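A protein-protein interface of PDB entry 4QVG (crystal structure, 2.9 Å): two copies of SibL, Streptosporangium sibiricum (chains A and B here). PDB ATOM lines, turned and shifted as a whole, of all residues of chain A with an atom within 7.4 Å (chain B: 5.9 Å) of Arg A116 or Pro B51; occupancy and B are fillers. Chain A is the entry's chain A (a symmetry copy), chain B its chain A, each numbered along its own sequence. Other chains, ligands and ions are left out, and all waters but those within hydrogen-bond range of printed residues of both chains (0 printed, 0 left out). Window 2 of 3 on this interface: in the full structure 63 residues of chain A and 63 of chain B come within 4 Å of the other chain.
Val A112 touches Gln B26.
Val A112 touches Leu B27.
Pro B51 touches Leu A115.
O of Gln B26 touches NH2 of Arg A116, at 3.8 Å.
Leu B27 touches Arg A116.
CD2 of Leu B50 touches CA of Arg A116, at 3.9 Å.
O of Arg A116 touches CD of Pro B51 (3.5 Å).
The side-chain hydroxyl of Ser B54 lies within hydrogen-bond range of the backbone carbonyl oxygen of Leu A115, 2.7 Å away.
O of Ala B45 lies within hydrogen-bond range of N of Leu B50 (2.9 Å).
The side-chain carboxylate of Glu A113 is in salt-bridge range of the guanidinium group of Arg A116, at 3.6 Å.
Printed residues of chain A that touch a printed residue of chain B: Val A112, Leu A115 and Arg A116.
Hydrophobic or aromatic side chains of chain B that line the printed part of chain A: Leu B27, Leu B50 and Pro B51.
Among the printed residues, no Asp or Glu carboxylate lies within 4 Å of a Lys or Arg side-chain nitrogen of the other chain.
No position is printed for both chains.
Of the 8 pairs that touch across the chains among the printed residues, none has its exchanged pair printed and touching as well.
Arg A116 touches just these residues of chain B: Gln B26 (3.8 Å), Leu B27 (3.3 Å), Leu B50 (3.9 Å) and Pro B51 (3.5 Å).
Of the printed residues of chain A, Leu B27 touches Val A112 (3.7 Å) and Arg A116 (3.3 Å).
Of the printed residues of chain A, Ser B54 touches Leu A115.
The nearest residue of chain B that does not touch Arg A116 is Ser B54 (4.7 Å).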
ATOM      1  N   ASP A 110     -22.241  15.399 -18.945  1.00  0.00           N
ATOM      2  CA  ASP A 110     -21.368  14.917 -17.877  1.00  0.00           C
ATOM      3  C   ASP A 110     -22.129  14.117 -16.805  1.00  0.00           C
ATOM      4  O   ASP A 110     -21.635  13.911 -15.698  1.00  0.00           O
ATOM      5  CB  ASP A 110     -20.667  16.112 -17.254  1.00  0.00           C
ATOM      6  CG  ASP A 110     -19.764  16.815 -18.229  1.00  0.00           C
ATOM      7  OD1 ASP A 110     -18.840  16.170 -18.769  1.00  0.00           O
ATOM      8  OD2 ASP A 110     -20.057  17.981 -18.566  1.00  0.00           O
ATOM      9  N   TYR A 111     -23.338  13.682 -17.150  1.00  0.00           N
ATOM     10  CA  TYR A 111     -24.188  12.811 -16.320  1.00  0.00           C
ATOM     11  C   TYR A 111     -23.469  11.522 -15.939  1.00  0.00           C
ATOM     12  O   TYR A 111     -23.490  11.110 -14.795  1.00  0.00           O
ATOM     13  CB  TYR A 111     -25.429  12.467 -17.119  1.00  0.00           C
ATOM     14  CG  TYR A 111     -26.537  11.718 -16.444  1.00  0.00           C
ATOM     15  CD1 TYR A 111     -27.108  12.172 -15.264  1.00  0.00           C
ATOM     16  CD2 TYR A 111     -27.071  10.574 -17.045  1.00  0.00           C
ATOM     17  CE1 TYR A 111     -28.180  11.491 -14.677  1.00  0.00           C
ATOM     18  CE2 TYR A 111     -28.134   9.875 -16.474  1.00  0.00           C
ATOM     19  CZ  TYR A 111     -28.690  10.340 -15.285  1.00  0.00           C
ATOM     20  OH  TYR A 111     -29.747   9.651 -14.730  1.00  0.00           O
ATOM     21  N   VAL A 112     -22.857  10.870 -16.917  1.00  0.00           N
ATOM     22  CA  VAL A 112     -22.179   9.611 -16.663  1.00  0.00           C
ATOM     23  C   VAL A 112     -21.116   9.795 -15.580  1.00  0.00           C
ATOM     24  O   VAL A 112     -21.098   9.073 -14.586  1.00  0.00           O
ATOM     25  CB  VAL A 112     -21.547   9.035 -17.953  1.00  0.00           C
ATOM     26  CG1 VAL A 112     -20.572   7.924 -17.627  1.00  0.00           C
ATOM     27  CG2 VAL A 112     -22.620   8.546 -18.870  1.00  0.00           C
ATOM     28  N   GLU A 113     -20.272  10.799 -15.742  1.00  0.00           N
ATOM     29  CA  GLU A 113     -19.217  11.010 -14.774  1.00  0.00           C
ATOM     30  C   GLU A 113     -19.813  11.473 -13.449  1.00  0.00           C
ATOM     31  O   GLU A 113     -19.275  11.161 -12.383  1.00  0.00           O
ATOM     32  CB  GLU A 113     -18.189  12.027 -15.298  1.00  0.00           C
ATOM     33  CG  GLU A 113     -16.937  12.148 -14.466  1.00  0.00           C
ATOM     34  CD  GLU A 113     -16.051  10.899 -14.516  1.00  0.00           C
ATOM     35  OE1 GLU A 113     -16.251  10.027 -15.424  1.00  0.00           O
ATOM     36  OE2 GLU A 113     -15.164  10.793 -13.621  1.00  0.00           O
ATOM     37  N   SER A 114     -20.956  12.155 -13.497  1.00  0.00           N
ATOM     38  CA  SER A 114     -21.583  12.604 -12.252  1.00  0.00           C
ATOM     39  C   SER A 114     -22.139  11.440 -11.475  1.00  0.00           C
ATOM     40  O   SER A 114     -22.043  11.414 -10.264  1.00  0.00           O
ATOM     41  CB  SER A 114     -22.708  13.589 -12.515  1.00  0.00           C
ATOM     42  OG  SER A 114     -22.176  14.847 -12.851  1.00  0.00           O
ATOM     43  N   LEU A 115     -22.668  10.448 -12.170  1.00  0.00           N
ATOM     44  CA  LEU A 115     -23.237   9.322 -11.482  1.00  0.00           C
ATOM     45  C   LEU A 115     -22.079   8.532 -10.854  1.00  0.00           C
ATOM     46  O   LEU A 115     -22.129   8.175  -9.682  1.00  0.00           O
ATOM     47  CB  LEU A 115     -24.022   8.448 -12.445  1.00  0.00           C
ATOM     48  CG  LEU A 115     -25.297   8.965 -13.123  1.00  0.00           C
ATOM     49  CD1 LEU A 115     -25.778   7.899 -14.117  1.00  0.00           C
ATOM     50  CD2 LEU A 115     -26.392   9.299 -12.165  1.00  0.00           C
ATOM     51  N   ARG A 116     -21.010   8.320 -11.613  1.00  0.00           N
ATOM     52  CA  ARG A 116     -19.843   7.601 -11.116  1.00  0.00           C
ATOM     53  C   ARG A 116     -19.229   8.218  -9.857  1.00  0.00           C
ATOM     54  O   ARG A 116     -19.008   7.545  -8.856  1.00  0.00           O
ATOM     55  CB  ARG A 116     -18.756   7.554 -12.180  1.00  0.00           C
ATOM     56  CG  ARG A 116     -18.894   6.437 -13.155  1.00  0.00           C
ATOM     57  CD  ARG A 116     -17.749   6.426 -14.145  1.00  0.00           C
ATOM     58  NE  ARG A 116     -18.020   5.491 -15.234  1.00  0.00           N
ATOM     59  CZ  ARG A 116     -17.709   5.726 -16.508  1.00  0.00           C
ATOM     60  NH1 ARG A 116     -17.083   6.858 -16.837  1.00  0.00           N
ATOM     61  NH2 ARG A 116     -17.998   4.820 -17.443  1.00  0.00           N
ATOM     62  N   THR A 117     -18.957   9.509  -9.905  1.00  0.00           N
ATOM     63  CA  THR A 117     -18.207  10.148  -8.849  1.00  0.00           C
ATOM     64  C   THR A 117     -19.131  10.647  -7.777  1.00  0.00           C
ATOM     65  O   THR A 117     -18.667  11.174  -6.787  1.00  0.00           O
ATOM     66  CB  THR A 117     -17.394  11.353  -9.333  1.00  0.00           C
ATOM     67  OG1 THR A 117     -18.269  12.478  -9.543  1.00  0.00           O
ATOM     68  CG2 THR A 117     -16.614  11.016 -10.591  1.00  0.00           C
ATOM     69  N   GLY A 118     -20.430  10.602  -8.026  1.00  0.00           N
ATOM     70  CA  GLY A 118     -21.407  11.072  -7.063  1.00  0.00           C
ATOM     71  C   GLY A 118     -21.326  12.571  -6.820  1.00  0.00           C
ATOM     72  O   GLY A 118     -21.913  13.102  -5.882  1.00  0.00           O
ATOM     73  N   GLN A 119     -20.509  13.248  -7.609  1.00  0.00           N
ATOM     74  CA  GLN A 119     -20.428  14.699  -7.553  1.00  0.00           C
ATOM     75  C   GLN A 119     -20.921  15.388  -8.843  1.00  0.00           C
ATOM     76  O   GLN A 119     -21.284  14.717  -9.825  1.00  0.00           O
ATOM     77  CB  GLN A 119     -19.014  15.087  -7.166  1.00  0.00           C
ATOM     78  CG  GLN A 119     -18.823  14.907  -5.667  1.00  0.00           C
ATOM     79  CD  GLN A 119     -17.422  15.179  -5.218  1.00  0.00           C
ATOM     80  OE1 GLN A 119     -16.477  14.985  -5.973  1.00  0.00           O
ATOM     81  NE2 GLN A 119     -17.271  15.657  -3.983  1.00  0.00           N
ATOM     82  N   THR A 297     -28.153  16.229 -10.738  1.00  0.00           N
ATOM     83  CA  THR A 297     -26.967  15.370 -10.604  1.00  0.00           C
ATOM     84  C   THR A 297     -25.724  16.009 -11.191  1.00  0.00           C
ATOM     85  O   THR A 297     -24.614  15.731 -10.756  1.00  0.00           O
ATOM     86  CB  THR A 297     -27.182  13.990 -11.312  1.00  0.00           C
ATOM     87  OG1 THR A 297     -28.152  13.220 -10.595  1.00  0.00           O
ATOM     88  CG2 THR A 297     -25.935  13.176 -11.324  1.00  0.00           C
ATOM     89  N   GLN B  26     -22.887   3.573 -21.564  1.00  0.00           N
ATOM     90  CA  GLN B  26     -21.513   3.762 -21.139  1.00  0.00           C
ATOM     91  C   GLN B  26     -21.182   2.968 -19.871  1.00  0.00           C
ATOM     92  O   GLN B  26     -20.048   2.521 -19.686  1.00  0.00           O
ATOM     93  CB  GLN B  26     -21.208   5.239 -20.916  1.00  0.00           C
ATOM     94  CG  GLN B  26     -21.127   6.109 -22.138  1.00  0.00           C
ATOM     95  CD  GLN B  26     -20.686   7.521 -21.764  1.00  0.00           C
ATOM     96  OE1 GLN B  26     -19.903   7.701 -20.835  1.00  0.00           O
ATOM     97  NE2 GLN B  26     -21.198   8.521 -22.468  1.00  0.00           N
ATOM     98  N   LEU B  27     -22.166   2.806 -18.991  1.00  0.00           N
ATOM     99  CA  LEU B  27     -21.913   2.152 -17.706  1.00  0.00           C
ATOM    100  C   LEU B  27     -22.237   0.673 -17.772  1.00  0.00           C
ATOM    101  O   LEU B  27     -22.062  -0.046 -16.795  1.00  0.00           O
ATOM    102  CB  LEU B  27     -22.727   2.790 -16.578  1.00  0.00           C
ATOM    103  CG  LEU B  27     -22.588   4.282 -16.260  1.00  0.00           C
ATOM    104  CD1 LEU B  27     -23.525   4.647 -15.101  1.00  0.00           C
ATOM    105  CD2 LEU B  27     -21.141   4.711 -15.944  1.00  0.00           C
ATOM    106  N   ALA B  45     -26.308  -1.587  -8.653  1.00  0.00           N
ATOM    107  CA  ALA B  45     -25.385  -0.614  -8.048  1.00  0.00           C
ATOM    108  C   ALA B  45     -24.012  -1.203  -7.796  1.00  0.00           C
ATOM    109  O   ALA B  45     -23.009  -0.534  -7.995  1.00  0.00           O
ATOM    110  CB  ALA B  45     -25.948  -0.082  -6.779  1.00  0.00           C
ATOM    111  N   ARG B  49     -20.447  -0.628 -10.059  1.00  0.00           N
ATOM    112  CA  ARG B  49     -19.598   0.158  -9.174  1.00  0.00           C
ATOM    113  C   ARG B  49     -20.077   1.609  -9.051  1.00  0.00           C
ATOM    114  O   ARG B  49     -19.287   2.551  -9.167  1.00  0.00           O
ATOM    115  CB  ARG B  49     -18.133   0.111  -9.635  1.00  0.00           C
ATOM    116  CG  ARG B  49     -17.494  -1.272  -9.572  1.00  0.00           C
ATOM    117  CD  ARG B  49     -17.407  -1.795  -8.127  1.00  0.00           C
ATOM    118  NE  ARG B  49     -16.226  -2.632  -7.916  1.00  0.00           N
ATOM    119  CZ  ARG B  49     -14.977  -2.167  -7.901  1.00  0.00           C
ATOM    120  NH1 ARG B  49     -14.738  -0.868  -8.100  1.00  0.00           N
ATOM    121  NH2 ARG B  49     -13.957  -2.998  -7.700  1.00  0.00           N
ATOM    122  N   LEU B  50     -21.369   1.777  -8.788  1.00  0.00           N
ATOM    123  CA  LEU B  50     -21.960   3.100  -8.620  1.00  0.00           C
ATOM    124  C   LEU B  50     -22.453   3.320  -7.204  1.00  0.00           C
ATOM    125  O   LEU B  50     -22.911   2.378  -6.526  1.00  0.00           O
ATOM    126  CB  LEU B  50     -23.171   3.263  -9.540  1.00  0.00           C
ATOM    127  CG  LEU B  50     -22.924   3.261 -11.035  1.00  0.00           C
ATOM    128  CD1 LEU B  50     -24.267   3.214 -11.734  1.00  0.00           C
ATOM    129  CD2 LEU B  50     -22.165   4.519 -11.405  1.00  0.00           C
ATOM    130  N   PRO B  51     -22.369   4.571  -6.746  1.00  0.00           N
ATOM    131  CA  PRO B  51     -23.042   4.946  -5.502  1.00  0.00           C
ATOM    132  C   PRO B  51     -24.489   4.563  -5.619  1.00  0.00           C
ATOM    133  O   PRO B  51     -25.044   4.720  -6.683  1.00  0.00           O
ATOM    134  CB  PRO B  51     -22.897   6.466  -5.477  1.00  0.00           C
ATOM    135  CG  PRO B  51     -21.608   6.708  -6.192  1.00  0.00           C
ATOM    136  CD  PRO B  51     -21.551   5.663  -7.291  1.00  0.00           C
ATOM    137  N   ARG B  52     -25.101   4.100  -4.552  1.00  0.00           N
ATOM    138  CA  ARG B  52     -26.479   3.639  -4.606  1.00  0.00           C
ATOM    139  C   ARG B  52     -27.388   4.775  -5.076  1.00  0.00           C
ATOM    140  O   ARG B  52     -28.335   4.550  -5.833  1.00  0.00           O
ATOM    141  CB  ARG B  52     -26.933   3.129  -3.234  1.00  0.00           C
ATOM    142  CG  ARG B  52     -28.394   2.751  -3.169  1.00  0.00           C
ATOM    143  CD  ARG B  52     -28.723   1.712  -4.221  1.00  0.00           C
ATOM    144  NE  ARG B  52     -30.173   1.558  -4.316  1.00  0.00           N
ATOM    145  CZ  ARG B  52     -30.892   0.686  -3.613  1.00  0.00           C
ATOM    146  NH1 ARG B  52     -30.306  -0.145  -2.748  1.00  0.00           N
ATOM    147  NH2 ARG B  52     -32.206   0.648  -3.782  1.00  0.00           N
ATOM    148  N   ARG B  53     -27.099   5.993  -4.618  1.00  0.00           N
ATOM    149  CA  ARG B  53     -27.894   7.147  -5.015  1.00  0.00           C
ATOM    150  C   ARG B  53     -27.869   7.273  -6.547  1.00  0.00           C
ATOM    151  O   ARG B  53     -28.914   7.367  -7.224  1.00  0.00           O
ATOM    152  CB  ARG B  53     -27.313   8.392  -4.384  1.00  0.00           C
ATOM    153  CG  ARG B  53     -28.256   9.484  -4.157  1.00  0.00           C
ATOM    154  CD  ARG B  53     -27.497  10.690  -3.683  1.00  0.00           C
ATOM    155  NE  ARG B  53     -27.103  11.516  -4.825  1.00  0.00           N
ATOM    156  CZ  ARG B  53     -27.845  12.506  -5.328  1.00  0.00           C
ATOM    157  NH1 ARG B  53     -29.033  12.809  -4.776  1.00  0.00           N
ATOM    158  NH2 ARG B  53     -27.384  13.198  -6.375  1.00  0.00           N
ATOM    159  N   SER B  54     -26.665   7.171  -7.090  1.00  0.00           N
ATOM    160  CA  SER B  54     -26.483   7.250  -8.511  1.00  0.00           C
ATOM    161  C   SER B  54     -27.256   6.157  -9.218  1.00  0.00           C
ATOM    162  O   SER B  54     -27.951   6.439 -10.200  1.00  0.00           O
ATOM    163  CB  SER B  54     -25.004   7.211  -8.857  1.00  0.00           C
ATOM    164  OG  SER B  54     -24.395   8.366  -8.316  1.00  0.00           O
ATOM    165  N   ALA B  55     -27.168   4.922  -8.729  1.00  0.00           N
ATOM    166  CA  ALA B  55     -27.892   3.840  -9.401  1.00  0.00           C
ATOM    167  C   ALA B  55     -29.406   4.029  -9.324  1.00  0.00           C
ATOM    168  O   ALA B  55     -30.107   3.754 -10.293  1.00  0.00           O
ATOM    169  CB  ALA B  55     -27.511   2.501  -8.848  1.00  0.00           C
ATOM    170  N   ASP B  56     -29.913   4.530  -8.203  1.00  0.00           N
ATOM    171  CA  ASP B  56     -31.348   4.714  -8.090  1.00  0.00           C
ATOM    172  C   ASP B  56     -31.871   5.726  -9.117  1.00  0.00           C
ATOM    173  O   ASP B  56     -32.878   5.486  -9.793  1.00  0.00           O
ATOM    174  CB  ASP B  56     -31.717   5.159  -6.673  1.00  0.00           C
ATOM    175  CG  ASP B  56     -31.698   4.003  -5.666  1.00  0.00           C
ATOM    176  OD1 ASP B  56     -31.785   2.833  -6.105  1.00  0.00           O
ATOM    177  OD2 ASP B  56     -31.653   4.262  -4.434  1.00  0.00           O
